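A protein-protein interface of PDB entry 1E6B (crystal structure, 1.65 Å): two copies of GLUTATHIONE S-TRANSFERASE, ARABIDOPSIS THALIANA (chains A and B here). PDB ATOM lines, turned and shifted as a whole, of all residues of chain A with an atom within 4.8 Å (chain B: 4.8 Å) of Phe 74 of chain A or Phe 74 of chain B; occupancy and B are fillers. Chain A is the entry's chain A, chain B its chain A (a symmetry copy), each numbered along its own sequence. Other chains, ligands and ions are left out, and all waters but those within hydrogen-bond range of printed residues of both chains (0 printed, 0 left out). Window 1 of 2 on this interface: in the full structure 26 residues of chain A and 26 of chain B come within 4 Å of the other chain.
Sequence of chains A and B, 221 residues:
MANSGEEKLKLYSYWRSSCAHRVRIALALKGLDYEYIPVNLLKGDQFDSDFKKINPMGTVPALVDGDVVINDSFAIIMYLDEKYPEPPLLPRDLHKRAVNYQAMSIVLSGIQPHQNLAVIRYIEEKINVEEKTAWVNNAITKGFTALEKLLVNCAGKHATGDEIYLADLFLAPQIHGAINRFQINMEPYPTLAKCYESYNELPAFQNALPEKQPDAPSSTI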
ATOM      1  N   ASP A  72      22.310 -37.689 -19.320  1.00  0.00           N
ATOM      2  CA  ASP A  72      22.533 -36.789 -20.440  1.00  0.00           C
ATOM      3  C   ASP A  72      23.809 -37.122 -21.200  1.00  0.00           C
ATOM      4  O   ASP A  72      24.913 -37.081 -20.671  1.00  0.00           O
ATOM      5  CB  ASP A  72      22.509 -35.292 -20.020  1.00  0.00           C
ATOM      6  CG  ASP A  72      22.637 -34.451 -21.280  1.00  0.00           C
ATOM      7  OD1 ASP A  72      21.613 -34.349 -22.002  1.00  0.00           O
ATOM      8  OD2 ASP A  72      23.748 -33.951 -21.554  1.00  0.00           O
ATOM      9  N   SER A  73      23.651 -37.391 -22.511  1.00  0.00           N
ATOM     10  CA  SER A  73      24.776 -37.742 -23.346  1.00  0.00           C
ATOM     11  C   SER A  73      25.901 -36.699 -23.321  1.00  0.00           C
ATOM     12  O   SER A  73      27.073 -37.073 -23.260  1.00  0.00           O
ATOM     13  CB  SER A  73      24.354 -38.043 -24.788  1.00  0.00           C
ATOM     14  OG  SER A  73      23.809 -36.930 -25.457  1.00  0.00           O
ATOM     15  N   PHE A  74      25.577 -35.423 -23.356  1.00  0.00           N
ATOM     16  CA  PHE A  74      26.589 -34.387 -23.375  1.00  0.00           C
ATOM     17  C   PHE A  74      27.266 -34.302 -22.005  1.00  0.00           C
ATOM     18  O   PHE A  74      28.502 -34.299 -21.991  1.00  0.00           O
ATOM     19  CB  PHE A  74      25.998 -33.019 -23.775  1.00  0.00           C
ATOM     20  CG  PHE A  74      27.035 -31.927 -23.629  1.00  0.00           C
ATOM     21  CD1 PHE A  74      28.163 -31.857 -24.444  1.00  0.00           C
ATOM     22  CD2 PHE A  74      26.851 -30.979 -22.622  1.00  0.00           C
ATOM     23  CE1 PHE A  74      29.131 -30.858 -24.240  1.00  0.00           C
ATOM     24  CE2 PHE A  74      27.785 -29.986 -22.442  1.00  0.00           C
ATOM     25  CZ  PHE A  74      28.939 -29.919 -23.252  1.00  0.00           C
ATOM     26  N   ALA A  75      26.491 -34.321 -20.924  1.00  0.00           N
ATOM     27  CA  ALA A  75      27.099 -34.245 -19.599  1.00  0.00           C
ATOM     28  C   ALA A  75      27.962 -35.507 -19.382  1.00  0.00           C
ATOM     29  O   ALA A  75      29.021 -35.362 -18.779  1.00  0.00           O
ATOM     30  CB  ALA A  75      26.029 -34.181 -18.517  1.00  0.00           C
ATOM     31  N   ILE A  76      27.517 -36.697 -19.812  1.00  0.00           N
ATOM     32  CA  ILE A  76      28.361 -37.873 -19.599  1.00  0.00           C
ATOM     33  C   ILE A  76      29.700 -37.758 -20.325  1.00  0.00           C
ATOM     34  O   ILE A  76      30.794 -38.073 -19.817  1.00  0.00           O
ATOM     35  CB  ILE A  76      27.650 -39.134 -20.152  1.00  0.00           C
ATOM     36  CG1 ILE A  76      26.429 -39.403 -19.295  1.00  0.00           C
ATOM     37  CG2 ILE A  76      28.596 -40.349 -20.160  1.00  0.00           C
ATOM     38  CD1 ILE A  76      25.463 -40.392 -19.892  1.00  0.00           C
ATOM     39  N   ILE A  77      29.626 -37.289 -21.578  1.00  0.00           N
ATOM     40  CA  ILE A  77      30.819 -37.176 -22.409  1.00  0.00           C
ATOM     41  C   ILE A  77      31.766 -36.144 -21.784  1.00  0.00           C
ATOM     42  O   ILE A  77      32.985 -36.363 -21.744  1.00  0.00           O
ATOM     43  CB  ILE A  77      30.439 -36.879 -23.870  1.00  0.00           C
ATOM     44  CG1 ILE A  77      29.803 -38.117 -24.537  1.00  0.00           C
ATOM     45  CG2 ILE A  77      31.612 -36.325 -24.684  1.00  0.00           C
ATOM     46  CD1 ILE A  77      29.099 -37.801 -25.847  1.00  0.00           C
ATOM     47  N   MET A  78      31.270 -35.015 -21.274  1.00  0.00           N
ATOM     48  CA  MET A  78      32.130 -34.006 -20.645  1.00  0.00           C
ATOM     49  C   MET A  78      32.725 -34.560 -19.366  1.00  0.00           C
ATOM     50  O   MET A  78      33.917 -34.350 -19.120  1.00  0.00           O
ATOM     51  CB  MET A  78      31.336 -32.718 -20.308  1.00  0.00           C
ATOM     52  CG  MET A  78      30.943 -32.014 -21.610  1.00  0.00           C
ATOM     53  SD  MET A  78      32.249 -31.510 -22.726  1.00  0.00           S
ATOM     54  CE  MET A  78      32.506 -32.909 -23.793  1.00  0.00           C
ATOM     55  N   TYR A 101      31.221 -26.988 -29.729  1.00  0.00           N
ATOM     56  CA  TYR A 101      30.029 -26.856 -28.881  1.00  0.00           C
ATOM     57  C   TYR A 101      28.775 -26.492 -29.678  1.00  0.00           C
ATOM     58  O   TYR A 101      27.653 -26.933 -29.326  1.00  0.00           O
ATOM     59  CB  TYR A 101      30.284 -25.780 -27.835  1.00  0.00           C
ATOM     60  CG  TYR A 101      31.338 -26.066 -26.782  1.00  0.00           C
ATOM     61  CD1 TYR A 101      31.340 -27.260 -26.071  1.00  0.00           C
ATOM     62  CD2 TYR A 101      32.312 -25.084 -26.525  1.00  0.00           C
ATOM     63  CE1 TYR A 101      32.285 -27.452 -25.084  1.00  0.00           C
ATOM     64  CE2 TYR A 101      33.262 -25.300 -25.533  1.00  0.00           C
ATOM     65  CZ  TYR A 101      33.244 -26.487 -24.844  1.00  0.00           C
ATOM     66  OH  TYR A 101      34.187 -26.715 -23.844  1.00  0.00           O
ATOM     67  N   MET A 104      27.533 -29.640 -31.419  1.00  0.00           N
ATOM     68  CA  MET A 104      26.908 -30.421 -30.387  1.00  0.00           C
ATOM     69  C   MET A 104      25.473 -29.904 -30.134  1.00  0.00           C
ATOM     70  O   MET A 104      24.509 -30.688 -30.210  1.00  0.00           O
ATOM     71  CB  MET A 104      27.750 -30.425 -29.102  1.00  0.00           C
ATOM     72  CG  MET A 104      27.142 -31.249 -27.958  1.00  0.00           C
ATOM     73  SD  MET A 104      25.769 -30.466 -27.124  1.00  0.00           S
ATOM     74  CE  MET A 104      26.506 -29.046 -26.316  1.00  0.00           C
ATOM     75  N   LEU A 108      22.004 -31.804 -30.388  1.00  0.00           N
ATOM     76  CA  LEU A 108      21.360 -32.041 -29.113  1.00  0.00           C
ATOM     77  C   LEU A 108      19.975 -31.423 -28.978  1.00  0.00           C
ATOM     78  O   LEU A 108      19.037 -32.064 -28.503  1.00  0.00           O
ATOM     79  CB  LEU A 108      22.225 -31.485 -27.965  1.00  0.00           C
ATOM     80  CG  LEU A 108      21.762 -31.592 -26.525  1.00  0.00           C
ATOM     81  CD1 LEU A 108      21.686 -33.043 -26.057  1.00  0.00           C
ATOM     82  CD2 LEU A 108      22.727 -30.853 -25.580  1.00  0.00           C
ATOM     83  N   LEU A 166      34.596 -33.567 -29.967  1.00  0.00           N
ATOM     84  CA  LEU A 166      33.179 -33.637 -29.524  1.00  0.00           C
ATOM     85  C   LEU A 166      32.184 -33.608 -30.683  1.00  0.00           C
ATOM     86  O   LEU A 166      31.236 -34.435 -30.695  1.00  0.00           O
ATOM     87  CB  LEU A 166      32.916 -32.493 -28.566  1.00  0.00           C
ATOM     88  CG  LEU A 166      31.453 -32.322 -28.102  1.00  0.00           C
ATOM     89  CD1 LEU A 166      31.102 -33.369 -27.048  1.00  0.00           C
ATOM     90  CD2 LEU A 166      31.257 -30.894 -27.587  1.00  0.00           C
ATOM     91  N   PHE A 170      28.887 -36.386 -31.819  1.00  0.00           N
ATOM     92  CA  PHE A 170      27.510 -35.969 -32.043  1.00  0.00           C
ATOM     93  C   PHE A 170      27.084 -36.211 -33.484  1.00  0.00           C
ATOM     94  O   PHE A 170      25.906 -36.626 -33.697  1.00  0.00           O
ATOM     95  CB  PHE A 170      27.273 -34.505 -31.563  1.00  0.00           C
ATOM     96  CG  PHE A 170      26.966 -34.557 -30.070  1.00  0.00           C
ATOM     97  CD1 PHE A 170      28.019 -34.747 -29.193  1.00  0.00           C
ATOM     98  CD2 PHE A 170      25.685 -34.451 -29.544  1.00  0.00           C
ATOM     99  CE1 PHE A 170      27.828 -34.816 -27.827  1.00  0.00           C
ATOM    100  CE2 PHE A 170      25.485 -34.539 -28.194  1.00  0.00           C
ATOM    101  CZ  PHE A 170      26.532 -34.726 -27.325  1.00  0.00           C
ATOM    102  N   ASP B  72      24.790 -19.778 -30.755  1.00  0.00           N
ATOM    103  CA  ASP B  72      24.370 -20.700 -29.711  1.00  0.00           C
ATOM    104  C   ASP B  72      24.713 -20.188 -28.320  1.00  0.00           C
ATOM    105  O   ASP B  72      25.869 -19.980 -27.969  1.00  0.00           O
ATOM    106  CB  ASP B  72      24.919 -22.139 -29.926  1.00  0.00           C
ATOM    107  CG  ASP B  72      24.326 -23.031 -28.848  1.00  0.00           C
ATOM    108  OD1 ASP B  72      23.127 -23.379 -28.993  1.00  0.00           O
ATOM    109  OD2 ASP B  72      25.034 -23.330 -27.865  1.00  0.00           O
ATOM    110  N   SER B  73      23.671 -20.052 -27.477  1.00  0.00           N
ATOM    111  CA  SER B  73      23.852 -19.556 -26.132  1.00  0.00           C
ATOM    112  C   SER B  73      24.874 -20.362 -25.321  1.00  0.00           C
ATOM    113  O   SER B  73      25.686 -19.768 -24.608  1.00  0.00           O
ATOM    114  CB  SER B  73      22.527 -19.448 -25.372  1.00  0.00           C
ATOM    115  OG  SER B  73      21.899 -20.691 -25.161  1.00  0.00           O
ATOM    116  N   PHE B  74      24.861 -21.676 -25.417  1.00  0.00           N
ATOM    117  CA  PHE B  74      25.771 -22.499 -24.648  1.00  0.00           C
ATOM    118  C   PHE B  74      27.191 -22.351 -25.200  1.00  0.00           C
ATOM    119  O   PHE B  74      28.088 -22.119 -24.383  1.00  0.00           O
ATOM    120  CB  PHE B  74      25.339 -23.980 -24.648  1.00  0.00           C
ATOM    121  CG  PHE B  74      26.388 -24.841 -23.979  1.00  0.00           C
ATOM    122  CD1 PHE B  74      26.665 -24.755 -22.617  1.00  0.00           C
ATOM    123  CD2 PHE B  74      27.110 -25.730 -24.776  1.00  0.00           C
ATOM    124  CE1 PHE B  74      27.687 -25.535 -22.045  1.00  0.00           C
ATOM    125  CE2 PHE B  74      28.090 -26.511 -24.210  1.00  0.00           C
ATOM    126  CZ  PHE B  74      28.389 -26.418 -22.834  1.00  0.00           C
ATOM    127  N   ALA B  75      27.356 -22.400 -26.520  1.00  0.00           N
ATOM    128  CA  ALA B  75      28.694 -22.261 -27.085  1.00  0.00           C
ATOM    129  C   ALA B  75      29.218 -20.846 -26.761  1.00  0.00           C
ATOM    130  O   ALA B  75      30.411 -20.742 -26.487  1.00  0.00           O
ATOM    131  CB  ALA B  75      28.663 -22.447 -28.596  1.00  0.00           C
ATOM    132  N   ILE B  76      28.386 -19.797 -26.829  1.00  0.00           N
ATOM    133  CA  ILE B  76      28.910 -18.469 -26.509  1.00  0.00           C
ATOM    134  C   ILE B  76      29.407 -18.381 -25.067  1.00  0.00           C
ATOM    135  O   ILE B  76      30.473 -17.828 -24.733  1.00  0.00           O
ATOM    136  CB  ILE B  76      27.791 -17.410 -26.670  1.00  0.00           C
ATOM    137  CG1 ILE B  76      27.437 -17.316 -28.140  1.00  0.00           C
ATOM    138  CG2 ILE B  76      28.233 -16.043 -26.121  1.00  0.00           C
ATOM    139  CD1 ILE B  76      26.156 -16.575 -28.421  1.00  0.00           C
ATOM    140  N   ILE B  77      28.603 -18.948 -24.156  1.00  0.00           N
ATOM    141  CA  ILE B  77      28.924 -18.893 -22.734  1.00  0.00           C
ATOM    142  C   ILE B  77      30.219 -19.678 -22.485  1.00  0.00           C
ATOM    143  O   ILE B  77      31.079 -19.229 -21.715  1.00  0.00           O
ATOM    144  CB  ILE B  77      27.730 -19.364 -21.888  1.00  0.00           C
ATOM    145  CG1 ILE B  77      26.591 -18.323 -21.913  1.00  0.00           C
ATOM    146  CG2 ILE B  77      28.131 -19.745 -20.460  1.00  0.00           C
ATOM    147  CD1 ILE B  77      25.268 -18.863 -21.393  1.00  0.00           C
ATOM    148  N   MET B  78      30.420 -20.839 -23.110  1.00  0.00           N
ATOM    149  CA  MET B  78      31.649 -21.617 -22.925  1.00  0.00           C
ATOM    150  C   MET B  78      32.828 -20.867 -23.511  1.00  0.00           C
ATOM    151  O   MET B  78      33.888 -20.829 -22.879  1.00  0.00           O
ATOM    152  CB  MET B  78      31.550 -23.004 -23.610  1.00  0.00           C
ATOM    153  CG  MET B  78      30.529 -23.864 -22.859  1.00  0.00           C
ATOM    154  SD  MET B  78      30.815 -24.192 -21.122  1.00  0.00           S
ATOM    155  CE  MET B  78      30.019 -22.853 -20.266  1.00  0.00           C
ATOM    156  N   TYR B 101      26.245 -29.333 -16.303  1.00  0.00           N
ATOM    157  CA  TYR B 101      25.982 -29.626 -17.719  1.00  0.00           C
ATOM    158  C   TYR B 101      24.617 -30.279 -17.943  1.00  0.00           C
ATOM    159  O   TYR B 101      23.964 -30.035 -18.987  1.00  0.00           O
ATOM    160  CB  TYR B 101      27.070 -30.553 -18.242  1.00  0.00           C
ATOM    161  CG  TYR B 101      28.478 -29.995 -18.334  1.00  0.00           C
ATOM    162  CD1 TYR B 101      28.728 -28.773 -18.945  1.00  0.00           C
ATOM    163  CD2 TYR B 101      29.535 -30.752 -17.798  1.00  0.00           C
ATOM    164  CE1 TYR B 101      30.032 -28.332 -19.056  1.00  0.00           C
ATOM    165  CE2 TYR B 101      30.840 -30.287 -17.911  1.00  0.00           C
ATOM    166  CZ  TYR B 101      31.063 -29.078 -18.520  1.00  0.00           C
ATOM    167  OH  TYR B 101      32.367 -28.601 -18.643  1.00  0.00           O
ATOM    168  N   MET B 104      21.961 -27.562 -17.722  1.00  0.00           N
ATOM    169  CA  MET B 104      22.056 -26.839 -18.960  1.00  0.00           C
ATOM    170  C   MET B 104      21.294 -27.600 -20.071  1.00  0.00           C
ATOM    171  O   MET B 104      20.401 -27.021 -20.719  1.00  0.00           O
ATOM    172  CB  MET B 104      23.520 -26.581 -19.346  1.00  0.00           C
ATOM    173  CG  MET B 104      23.694 -25.805 -20.660  1.00  0.00           C
ATOM    174  SD  MET B 104      23.416 -26.771 -22.138  1.00  0.00           S
ATOM    175  CE  MET B 104      24.756 -27.961 -22.136  1.00  0.00           C
ATOM    176  N   LEU B 108      18.274 -26.418 -22.348  1.00  0.00           N
ATOM    177  CA  LEU B 108      18.619 -26.213 -23.738  1.00  0.00           C
ATOM    178  C   LEU B 108      17.834 -27.071 -24.720  1.00  0.00           C
ATOM    179  O   LEU B 108      17.356 -26.586 -25.747  1.00  0.00           O
ATOM    180  CB  LEU B 108      20.116 -26.508 -23.967  1.00  0.00           C
ATOM    181  CG  LEU B 108      20.727 -26.385 -25.348  1.00  0.00           C
ATOM    182  CD1 LEU B 108      20.711 -24.944 -25.853  1.00  0.00           C
ATOM    183  CD2 LEU B 108      22.193 -26.855 -25.345  1.00  0.00           C
ATOM    184  N   LEU B 166      27.257 -22.269 -14.354  1.00  0.00           N
ATOM    185  CA  LEU B 166      26.524 -22.437 -15.636  1.00  0.00           C
ATOM    186  C   LEU B 166      25.039 -22.740 -15.444  1.00  0.00           C
ATOM    187  O   LEU B 166      24.194 -22.112 -16.131  1.00  0.00           O
ATOM    188  CB  LEU B 166      27.193 -23.536 -16.435  1.00  0.00           C
ATOM    189  CG  LEU B 166      26.487 -23.947 -17.745  1.00  0.00           C
ATOM    190  CD1 LEU B 166      26.743 -22.910 -18.836  1.00  0.00           C
ATOM    191  CD2 LEU B 166      26.963 -25.343 -18.151  1.00  0.00           C
ATOM    192  N   PHE B 170      21.384 -20.730 -17.019  1.00  0.00           N
ATOM    193  CA  PHE B 170      20.325 -21.418 -17.746  1.00  0.00           C
ATOM    194  C   PHE B 170      19.008 -21.367 -16.984  1.00  0.00           C
ATOM    195  O   PHE B 170      17.940 -21.201 -17.647  1.00  0.00           O
ATOM    196  CB  PHE B 170      20.753 -22.860 -18.150  1.00  0.00           C
ATOM    197  CG  PHE B 170      21.524 -22.756 -19.463  1.00  0.00           C
ATOM    198  CD1 PHE B 170      22.832 -22.306 -19.419  1.00  0.00           C
ATOM    199  CD2 PHE B 170      20.977 -23.064 -20.702  1.00  0.00           C
ATOM    200  CE1 PHE B 170      23.596 -22.173 -20.561  1.00  0.00           C
ATOM    201  CE2 PHE B 170      21.721 -22.916 -21.839  1.00  0.00           C
ATOM    202  CZ  PHE B 170      23.020 -22.470 -21.794  1.00  0.00           C
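OD2 of Asp 72 of chain A is in hydrogen-bond range of N of Phe 74 of chain A, 3.0 Å away.
OD2 of Asp 72 of chain A lies within hydrogen-bond range of N of Ala 75 of chain A, 2.8 Å away.
The backbone NH (N) of Phe 74 of chain B sits at hydrogen-bond distance from the side-chain carboxylate (OD2) of Asp 72 of chain B (3.0 Å).
OD2 of Asp 72 of chain B is in hydrogen-bond range of N of Ala 75 of chain B.
Phe 74 of chain B touches Phe 74 of chain A (CZ to CZ, 3.6 Å).
Tyr 101 of chain B touches Phe 74 of chain A (CD1 to CE2, 3.8 Å).
CE of Met 104 of chain B touches CE2 of Phe 74 of chain A, 3.7 Å away.
Ala 75 of chain A touches Tyr 101 of chain B (CB to CB, 3.8 Å).
CB of Met 78 of chain A touches CE2 of Tyr 101 of chain B (3.4 Å).
Phe 74 of chain B touches Tyr 101 of chain A.
CB of Tyr 101 of chain A touches CB of Ala 75 of chain B, 3.8 Å away.
Tyr 101 of chain A touches Met 78 of chain B (CE2 to CB, 3.4 Å).
Met 104 of chain A touches Phe 74 of chain B (CE to CE2, 3.7 Å).
Hydrophobic or aromatic side chains of chain B within 4 Å of the printed part of chain A: Phe 74, Ala 75, Met 78, Tyr 101 and Met 104.
Phe 74 of chain A touches just these residues of chain B: Phe 74, Tyr 101 and Met 104.
Of chain A, only Phe 74 (3.6 Å), Tyr 101 (3.8 Å) and Met 104 (3.7 Å) come within 4 Å of Phe 74 of chain B.
Printed residues of chain A within 4 Å of Met 104 of chain B: Phe 74.
Printed residues of chain B within 4 Å of Ala 75 of chain A: Tyr 101 (3.8 Å).
Printed residues of chain A within 4 Å of Ala 75 of chain B: Tyr 101.
Asp 72 of chain B touches none of the printed residues of chain A.
The nearest printed residue of chain B that does not touch Phe 74 of chain A is Met 78 of chain B (6.3 Å).
The nearest printed residue of chain A that does not touch Phe 74 of chain B is Met 78 of chain A (6.3 Å).
Phe 74 of chain A touches Tyr 101 of chain B, and with the chains exchanged Tyr 101 of chain A touches Phe 74 of chain B.
Phe 74 of chain A touches Met 104 of chain B, and with the chains exchanged Met 104 of chain A touches Phe 74 of chain B.
Ala 75 of chain A touches Tyr 101 of chain B, and with the chains exchanged Tyr 101 of chain A touches Ala 75 of chain B.
Met 78 of chain A touches Tyr 101 of chain B, and with the chains exchanged Tyr 101 of chain A touches Met 78 of chain B.
Positions printed for both chains: 72, 73, 74, 75, 76, 77, 78, 101, 104, 108, 166 and 170.
Of the 9 pairs that touch across the chains among the printed residues, 9 have their exchanged pair printed and touching as well.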
